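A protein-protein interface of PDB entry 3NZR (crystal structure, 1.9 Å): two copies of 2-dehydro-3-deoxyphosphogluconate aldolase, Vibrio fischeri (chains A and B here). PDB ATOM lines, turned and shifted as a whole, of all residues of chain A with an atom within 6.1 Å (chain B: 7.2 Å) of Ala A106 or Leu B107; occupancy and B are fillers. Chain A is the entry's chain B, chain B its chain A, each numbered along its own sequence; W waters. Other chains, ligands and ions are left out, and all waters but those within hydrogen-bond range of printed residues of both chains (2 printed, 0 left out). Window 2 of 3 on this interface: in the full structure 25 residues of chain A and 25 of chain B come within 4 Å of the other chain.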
ATOM      1  N   VAL A 101     -32.524 -32.764 -24.632  1.00  0.00           N
ATOM      2  CA  VAL A 101     -32.857 -33.533 -23.367  1.00  0.00           C
ATOM      3  C   VAL A 101     -32.537 -32.661 -22.147  1.00  0.00           C
ATOM      4  O   VAL A 101     -33.393 -32.422 -21.297  1.00  0.00           O
ATOM      5  CB  VAL A 101     -32.122 -34.904 -23.300  1.00  0.00           C
ATOM      6  CG1 VAL A 101     -32.399 -35.607 -21.946  1.00  0.00           C
ATOM      7  CG2 VAL A 101     -32.669 -35.874 -24.348  1.00  0.00           C
ATOM      8  N   ALA A 102     -31.328 -32.129 -22.110  1.00  0.00           N
ATOM      9  CA  ALA A 102     -30.893 -31.284 -21.006  1.00  0.00           C
ATOM     10  C   ALA A 102     -31.690 -30.023 -20.855  1.00  0.00           C
ATOM     11  O   ALA A 102     -31.973 -29.601 -19.729  1.00  0.00           O
ATOM     12  CB  ALA A 102     -29.399 -30.974 -21.098  1.00  0.00           C
ATOM     13  N   THR A 103     -31.990 -29.363 -21.946  1.00  0.00           N
ATOM     14  CA  THR A 103     -32.898 -28.181 -21.922  1.00  0.00           C
ATOM     15  C   THR A 103     -34.252 -28.414 -21.317  1.00  0.00           C
ATOM     16  O   THR A 103     -34.661 -27.693 -20.459  1.00  0.00           O
ATOM     17  CB  THR A 103     -33.031 -27.570 -23.277  1.00  0.00           C
ATOM     18  OG1 THR A 103     -31.701 -27.351 -23.858  1.00  0.00           O
ATOM     19  CG2 THR A 103     -33.835 -26.229 -23.202  1.00  0.00           C
ATOM     20  N   SER A 104     -34.926 -29.467 -21.740  1.00  0.00           N
ATOM     21  CA  SER A 104     -36.160 -29.783 -21.190  1.00  0.00           C
ATOM     22  C   SER A 104     -36.082 -30.156 -19.754  1.00  0.00           C
ATOM     23  O   SER A 104     -37.015 -29.820 -19.000  1.00  0.00           O
ATOM     24  CB  SER A 104     -36.800 -30.924 -21.954  1.00  0.00           C
ATOM     25  OG  SER A 104     -37.279 -30.419 -23.163  1.00  0.00           O
ATOM     26  N   ARG A 105     -35.059 -30.917 -19.340  1.00  0.00           N
ATOM     27  CA  ARG A 105     -34.993 -31.242 -17.933  1.00  0.00           C
ATOM     28  C   ARG A 105     -34.766 -29.951 -17.128  1.00  0.00           C
ATOM     29  O   ARG A 105     -35.396 -29.774 -16.042  1.00  0.00           O
ATOM     30  CB  ARG A 105     -33.871 -32.268 -17.636  1.00  0.00           C
ATOM     31  CG  ARG A 105     -33.582 -32.501 -16.153  1.00  0.00           C
ATOM     32  CD  ARG A 105     -34.762 -33.170 -15.464  1.00  0.00           C
ATOM     33  NE  ARG A 105     -34.984 -34.512 -16.056  1.00  0.00           N
ATOM     34  CZ  ARG A 105     -36.150 -35.128 -16.082  1.00  0.00           C
ATOM     35  NH1 ARG A 105     -37.193 -34.552 -15.565  1.00  0.00           N
ATOM     36  NH2 ARG A 105     -36.256 -36.371 -16.609  1.00  0.00           N
ATOM     37  N   ALA A 106     -33.804 -29.112 -17.544  1.00  0.00           N
ATOM     38  CA  ALA A 106     -33.572 -27.829 -16.831  1.00  0.00           C
ATOM     39  C   ALA A 106     -34.796 -26.935 -16.713  1.00  0.00           C
ATOM     40  O   ALA A 106     -35.144 -26.500 -15.615  1.00  0.00           O
ATOM     41  CB  ALA A 106     -32.451 -27.082 -17.500  1.00  0.00           C
ATOM     42  N   LEU A 107     -35.542 -26.731 -17.803  1.00  0.00           N
ATOM     43  CA  LEU A 107     -36.737 -25.906 -17.757  1.00  0.00           C
ATOM     44  C   LEU A 107     -37.930 -26.562 -17.028  1.00  0.00           C
ATOM     45  O   LEU A 107     -38.812 -25.885 -16.549  1.00  0.00           O
ATOM     46  CB  LEU A 107     -37.130 -25.440 -19.157  1.00  0.00           C
ATOM     47  CG  LEU A 107     -36.041 -24.642 -19.950  1.00  0.00           C
ATOM     48  CD1 LEU A 107     -36.642 -23.994 -21.214  1.00  0.00           C
ATOM     49  CD2 LEU A 107     -35.298 -23.596 -19.161  1.00  0.00           C
ATOM     50  N   ALA A 108     -37.973 -27.866 -16.973  1.00  0.00           N
ATOM     51  CA  ALA A 108     -39.053 -28.532 -16.264  1.00  0.00           C
ATOM     52  C   ALA A 108     -38.852 -28.263 -14.770  1.00  0.00           C
ATOM     53  O   ALA A 108     -39.851 -28.151 -14.022  1.00  0.00           O
ATOM     54  CB  ALA A 108     -39.003 -30.002 -16.566  1.00  0.00           C
ATOM     55  N   GLY A 109     -37.590 -28.193 -14.320  1.00  0.00           N
ATOM     56  CA  GLY A 109     -37.259 -27.827 -12.959  1.00  0.00           C
ATOM     57  C   GLY A 109     -37.535 -28.885 -11.893  1.00  0.00           C
ATOM     58  O   GLY A 109     -37.577 -28.575 -10.668  1.00  0.00           O
ATOM     59  N   GLN A 110     -37.757 -30.125 -12.338  1.00  0.00           N
ATOM     60  CA  GLN A 110     -37.863 -31.228 -11.413  1.00  0.00           C
ATOM     61  C   GLN A 110     -37.481 -32.530 -12.139  1.00  0.00           C
ATOM     62  O   GLN A 110     -37.294 -32.510 -13.370  1.00  0.00           O
ATOM     63  CB  GLN A 110     -39.278 -31.289 -10.829  1.00  0.00           C
ATOM     64  CG  GLN A 110     -40.399 -30.910 -11.759  1.00  0.00           C
ATOM     65  CD  GLN A 110     -40.702 -31.901 -12.848  1.00  0.00           C
ATOM     66  OE1 GLN A 110     -40.304 -33.082 -12.787  1.00  0.00           O
ATOM     67  NE2 GLN A 110     -41.431 -31.439 -13.860  1.00  0.00           N
ATOM     68  N   MET B  80     -22.431 -30.232 -12.870  1.00  0.00           N
ATOM     69  CA  MET B  80     -23.661 -29.658 -12.347  1.00  0.00           C
ATOM     70  C   MET B  80     -23.375 -28.477 -11.430  1.00  0.00           C
ATOM     71  O   MET B  80     -24.087 -27.483 -11.413  1.00  0.00           O
ATOM     72  CB  MET B  80     -24.529 -30.694 -11.680  1.00  0.00           C
ATOM     73  CG  MET B  80     -25.839 -30.134 -11.179  1.00  0.00           C
ATOM     74  SD  MET B  80     -27.032 -29.193 -12.542  1.00  0.00           S
ATOM     75  CE  MET B  80     -27.786 -30.879 -13.397  1.00  0.00           C
ATOM     76  N   SER B  83     -22.956 -25.390 -13.441  1.00  0.00           N
ATOM     77  CA  SER B  83     -24.141 -24.887 -13.935  1.00  0.00           C
ATOM     78  C   SER B  83     -24.867 -24.155 -12.836  1.00  0.00           C
ATOM     79  O   SER B  83     -25.345 -23.038 -13.097  1.00  0.00           O
ATOM     80  CB  SER B  83     -25.060 -26.026 -14.420  1.00  0.00           C
ATOM     81  OG  SER B  83     -24.588 -26.679 -15.617  1.00  0.00           O
ATOM     82  N   LEU B  84     -24.976 -24.736 -11.641  1.00  0.00           N
ATOM     83  CA  LEU B  84     -25.734 -24.100 -10.538  1.00  0.00           C
ATOM     84  C   LEU B  84     -25.004 -22.830 -10.070  1.00  0.00           C
ATOM     85  O   LEU B  84     -25.604 -21.813  -9.810  1.00  0.00           O
ATOM     86  CB  LEU B  84     -25.833 -25.034  -9.345  1.00  0.00           C
ATOM     87  CG  LEU B  84     -26.694 -26.252  -9.612  1.00  0.00           C
ATOM     88  CD1 LEU B  84     -26.591 -27.224  -8.440  1.00  0.00           C
ATOM     89  CD2 LEU B  84     -28.131 -25.809  -9.763  1.00  0.00           C
ATOM     90  N   ILE B  85     -23.689 -22.886  -9.959  1.00  0.00           N
ATOM     91  CA  ILE B  85     -22.909 -21.638  -9.675  1.00  0.00           C
ATOM     92  C   ILE B  85     -23.141 -20.524 -10.701  1.00  0.00           C
ATOM     93  O   ILE B  85     -23.367 -19.345 -10.340  1.00  0.00           O
ATOM     94  CB  ILE B  85     -21.408 -21.966  -9.621  1.00  0.00           C
ATOM     95  CG1 ILE B  85     -21.088 -22.802  -8.375  1.00  0.00           C
ATOM     96  CG2 ILE B  85     -20.524 -20.680  -9.614  1.00  0.00           C
ATOM     97  CD1 ILE B  85     -19.682 -23.375  -8.412  1.00  0.00           C
ATOM     98  N   SER B  86     -23.042 -20.846 -11.982  1.00  0.00           N
ATOM     99  CA  SER B  86     -23.182 -19.864 -13.029  1.00  0.00           C
ATOM    100  C   SER B  86     -24.577 -19.239 -13.050  1.00  0.00           C
ATOM    101  O   SER B  86     -24.758 -18.068 -13.349  1.00  0.00           O
ATOM    102  CB  SER B  86     -22.823 -20.475 -14.399  1.00  0.00           C
ATOM    103  OG  SER B  86     -21.478 -21.013 -14.393  1.00  0.00           O
ATOM    104  N   GLN B  87     -25.602 -20.035 -12.760  1.00  0.00           N
ATOM    105  CA  GLN B  87     -26.939 -19.528 -12.622  1.00  0.00           C
ATOM    106  C   GLN B  87     -26.925 -18.282 -11.727  1.00  0.00           C
ATOM    107  O   GLN B  87     -27.507 -17.273 -12.115  1.00  0.00           O
ATOM    108  CB  GLN B  87     -27.871 -20.580 -12.044  1.00  0.00           C
ATOM    109  CG  GLN B  87     -29.334 -20.108 -11.858  1.00  0.00           C
ATOM    110  CD  GLN B  87     -30.269 -21.255 -11.577  1.00  0.00           C
ATOM    111  OE1 GLN B  87     -29.903 -22.203 -10.908  1.00  0.00           O
ATOM    112  NE2 GLN B  87     -31.482 -21.182 -12.098  1.00  0.00           N
ATOM    113  N   HIS B  88     -26.281 -18.355 -10.569  1.00  0.00           N
ATOM    114  CA  HIS B  88     -26.286 -17.233  -9.598  1.00  0.00           C
ATOM    115  C   HIS B  88     -25.206 -16.219  -9.855  1.00  0.00           C
ATOM    116  O   HIS B  88     -25.417 -15.049  -9.646  1.00  0.00           O
ATOM    117  CB  HIS B  88     -26.157 -17.756  -8.191  1.00  0.00           C
ATOM    118  CG  HIS B  88     -27.270 -18.650  -7.813  1.00  0.00           C
ATOM    119  ND1 HIS B  88     -27.085 -19.799  -7.076  1.00  0.00           N
ATOM    120  CD2 HIS B  88     -28.598 -18.577  -8.085  1.00  0.00           C
ATOM    121  CE1 HIS B  88     -28.264 -20.384  -6.892  1.00  0.00           C
ATOM    122  NE2 HIS B  88     -29.196 -19.664  -7.497  1.00  0.00           N
ATOM    123  N   GLN B  90     -23.877 -15.410 -12.957  1.00  0.00           N
ATOM    124  CA  GLN B  90     -24.056 -14.715 -14.249  1.00  0.00           C
ATOM    125  C   GLN B  90     -22.689 -14.174 -14.747  1.00  0.00           C
ATOM    126  O   GLN B  90     -22.518 -12.980 -14.950  1.00  0.00           O
ATOM    127  CB  GLN B  90     -25.083 -13.569 -14.145  1.00  0.00           C
ATOM    128  CG  GLN B  90     -26.522 -14.069 -13.800  1.00  0.00           C
ATOM    129  CD  GLN B  90     -27.220 -14.795 -14.968  1.00  0.00           C
ATOM    130  OE1 GLN B  90     -27.355 -14.262 -16.055  1.00  0.00           O
ATOM    131  NE2 GLN B  90     -27.711 -15.965 -14.704  1.00  0.00           N
ATOM    132  N   ILE B  94     -18.485 -19.569 -19.077  1.00  0.00           N
ATOM    133  CA  ILE B  94     -18.715 -20.800 -18.376  1.00  0.00           C
ATOM    134  C   ILE B  94     -17.998 -21.954 -19.082  1.00  0.00           C
ATOM    135  O   ILE B  94     -18.145 -22.089 -20.289  1.00  0.00           O
ATOM    136  CB  ILE B  94     -20.191 -21.073 -18.392  1.00  0.00           C
ATOM    137  CG1 ILE B  94     -20.949 -19.979 -17.647  1.00  0.00           C
ATOM    138  CG2 ILE B  94     -20.530 -22.389 -17.677  1.00  0.00           C
ATOM    139  CD1 ILE B  94     -22.478 -19.937 -17.909  1.00  0.00           C
ATOM    140  N   VAL B 101     -23.362 -28.461 -21.493  1.00  0.00           N
ATOM    141  CA  VAL B 101     -23.577 -27.218 -22.218  1.00  0.00           C
ATOM    142  C   VAL B 101     -24.999 -26.680 -22.157  1.00  0.00           C
ATOM    143  O   VAL B 101     -25.245 -25.491 -21.763  1.00  0.00           O
ATOM    144  CB  VAL B 101     -23.121 -27.410 -23.670  1.00  0.00           C
ATOM    145  CG1 VAL B 101     -23.416 -26.140 -24.508  1.00  0.00           C
ATOM    146  CG2 VAL B 101     -21.622 -27.737 -23.640  1.00  0.00           C
ATOM    147  N   ALA B 102     -25.978 -27.560 -22.444  1.00  0.00           N
ATOM    148  CA  ALA B 102     -27.342 -27.146 -22.510  1.00  0.00           C
ATOM    149  C   ALA B 102     -27.858 -26.776 -21.144  1.00  0.00           C
ATOM    150  O   ALA B 102     -28.641 -25.826 -21.011  1.00  0.00           O
ATOM    151  CB  ALA B 102     -28.259 -28.320 -23.174  1.00  0.00           C
ATOM    152  N   THR B 103     -27.500 -27.571 -20.123  1.00  0.00           N
ATOM    153  CA  THR B 103     -27.919 -27.254 -18.801  1.00  0.00           C
ATOM    154  C   THR B 103     -27.432 -25.887 -18.332  1.00  0.00           C
ATOM    155  O   THR B 103     -28.185 -25.113 -17.737  1.00  0.00           O
ATOM    156  CB  THR B 103     -27.365 -28.274 -17.821  1.00  0.00           C
ATOM    157  OG1 THR B 103     -27.756 -29.603 -18.205  1.00  0.00           O
ATOM    158  CG2 THR B 103     -27.898 -27.953 -16.396  1.00  0.00           C
ATOM    159  N   SER B 104     -26.164 -25.601 -18.538  1.00  0.00           N
ATOM    160  CA  SER B 104     -25.627 -24.303 -18.208  1.00  0.00           C
ATOM    161  C   SER B 104     -26.311 -23.152 -18.967  1.00  0.00           C
ATOM    162  O   SER B 104     -26.574 -22.161 -18.412  1.00  0.00           O
ATOM    163  CB  SER B 104     -24.133 -24.274 -18.429  1.00  0.00           C
ATOM    164  OG  SER B 104     -23.456 -24.945 -17.429  1.00  0.00           O
ATOM    165  N   ARG B 105     -26.557 -23.326 -20.247  1.00  0.00           N
ATOM    166  CA  ARG B 105     -27.263 -22.329 -21.007  1.00  0.00           C
ATOM    167  C   ARG B 105     -28.675 -22.132 -20.473  1.00  0.00           C
ATOM    168  O   ARG B 105     -29.125 -21.050 -20.408  1.00  0.00           O
ATOM    169  CB  ARG B 105     -27.307 -22.598 -22.488  1.00  0.00           C
ATOM    170  CG  ARG B 105     -28.150 -21.611 -23.299  1.00  0.00           C
ATOM    171  CD  ARG B 105     -27.564 -20.247 -23.344  1.00  0.00           C
ATOM    172  NE  ARG B 105     -26.314 -20.251 -24.029  1.00  0.00           N
ATOM    173  CZ  ARG B 105     -25.332 -19.375 -23.887  1.00  0.00           C
ATOM    174  NH1 ARG B 105     -25.439 -18.365 -23.092  1.00  0.00           N
ATOM    175  NH2 ARG B 105     -24.251 -19.527 -24.559  1.00  0.00           N
ATOM    176  N   ALA B 106     -29.335 -23.198 -20.095  1.00  0.00           N
ATOM    177  CA  ALA B 106     -30.705 -23.072 -19.644  1.00  0.00           C
ATOM    178  C   ALA B 106     -30.763 -22.359 -18.319  1.00  0.00           C
ATOM    179  O   ALA B 106     -31.488 -21.417 -18.163  1.00  0.00           O
ATOM    180  CB  ALA B 106     -31.408 -24.392 -19.611  1.00  0.00           C
ATOM    181  N   LEU B 107     -29.938 -22.769 -17.383  1.00  0.00           N
ATOM    182  CA  LEU B 107     -29.961 -22.140 -16.053  1.00  0.00           C
ATOM    183  C   LEU B 107     -29.313 -20.754 -16.037  1.00  0.00           C
ATOM    184  O   LEU B 107     -29.599 -20.008 -15.157  1.00  0.00           O
ATOM    185  CB  LEU B 107     -29.291 -23.010 -14.995  1.00  0.00           C
ATOM    186  CG  LEU B 107     -29.857 -24.449 -14.879  1.00  0.00           C
ATOM    187  CD1 LEU B 107     -29.108 -25.088 -13.720  1.00  0.00           C
ATOM    188  CD2 LEU B 107     -31.388 -24.505 -14.668  1.00  0.00           C
ATOM    189  N   ALA B 108     -28.472 -20.427 -16.998  1.00  0.00           N
ATOM    190  CA  ALA B 108     -27.984 -19.046 -17.173  1.00  0.00           C
ATOM    191  C   ALA B 108     -29.115 -18.114 -17.540  1.00  0.00           C
ATOM    192  O   ALA B 108     -29.144 -16.933 -17.094  1.00  0.00           O
ATOM    193  CB  ALA B 108     -26.978 -18.968 -18.201  1.00  0.00           C
ATOM    194  N   GLY B 109     -30.056 -18.629 -18.336  1.00  0.00           N
ATOM    195  CA  GLY B 109     -31.261 -17.891 -18.652  1.00  0.00           C
ATOM    196  C   GLY B 109     -31.095 -16.741 -19.633  1.00  0.00           C
ATOM    197  O   GLY B 109     -32.030 -15.965 -19.761  1.00  0.00           O
ATOM    198  N   GLN B 110     -29.934 -16.645 -20.315  1.00  0.00           N
ATOM    199  CA  GLN B 110     -29.713 -15.681 -21.415  1.00  0.00           C
ATOM    200  C   GLN B 110     -28.676 -16.186 -22.402  1.00  0.00           C
ATOM    201  O   GLN B 110     -27.964 -17.145 -22.129  1.00  0.00           O
ATOM    202  CB  GLN B 110     -29.237 -14.333 -20.903  1.00  0.00           C
ATOM    203  CG  GLN B 110     -28.444 -14.381 -19.672  1.00  0.00           C
ATOM    204  CD  GLN B 110     -27.027 -14.735 -19.876  1.00  0.00           C
ATOM    205  OE1 GLN B 110     -26.518 -14.712 -21.017  1.00  0.00           O
ATOM    206  NE2 GLN B 110     -26.337 -15.031 -18.769  1.00  0.00           N
HETATM  207  O   HOH W   1     -30.499 -30.112 -17.461  1.00  0.00           O
HETATM  208  O   HOH W   2     -30.357 -25.068 -23.117  1.00  0.00           O
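Of the printed residues of chain B, Ala A102 touches Ala B102 (3.6 Å) and Thr B103 (3.6 Å). Printed residues of chain B within 4 Å of Thr A103: Ala B102 (3.6 Å). Ala A106 touches just these residues of chain B: Ala B106 (3.6 Å) and Leu B107 (3.97 Å). Of the printed residues of chain B, Leu A107 touches Ala B106 (3.996 Å). Ala A108 touches none of the printed residues of chain B. Of the printed residues of chain A, Thr B103 touches Ala A102 (3.6 Å). Of the printed residues of chain A, Leu B107 touches Ala A106 (3.97 Å). The nearest residue of chain B that does not touch Ala A106 is Thr B103 (4.7 Å). The nearest residue of chain A that does not touch Leu B107 is Leu A107 (5.7 Å). The nearest printed residue of chain A that does not touch Ala B106 is Thr A103 (4.7 Å).
Of the 19 printed residues of chain B, 4 touch a printed residue of chain A. Hydrophobic or aromatic side chains of chain B within 4 Å of the printed part of chain A: Ala B102, Ala B106 and Leu B107. Along chain B the printed residues that touch a printed residue of chain A span positions 102 to 107. Among the printed residues, 6 pairs touch across the chains. Among the printed residues, no Asp or Glu carboxylate lies within 4 Å of a Lys or Arg side-chain nitrogen of the other chain.
Ala A102 touches its own counterpart, Ala B102. Ala A102 touches Thr B103, and with the chains exchanged Thr A103 touches Ala B102. Ala A106 touches its own counterpart, Ala B106. Ala A106 touches Leu B107, and with the chains exchanged Leu A107 touches Ala B106.
Water W2 lies within hydrogen-bond range of the side-chain hydroxyl of Thr A103 and the backbone carbonyl oxygen of Ala B102. Water W1 lies within hydrogen-bond range of the backbone carbonyl oxygen (O) of Ala A102 (2.8 Å), the side-chain hydroxyl (OG1) of Thr B103 (2.9 Å) and the backbone NH (N) of Ala A106 (3.5 Å).
CB of Ala A102 touches CB of Ala B102, 3.6 Å away. CB of Ala A102 touches OG1 of Thr B103 (3.6 Å). Thr A103 touches Ala B102. Ala A106 touches Ala B106. Leu B107 touches Ala A106. Ala B106 touches Leu A107 (CB to CD2, 3.996 Å).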
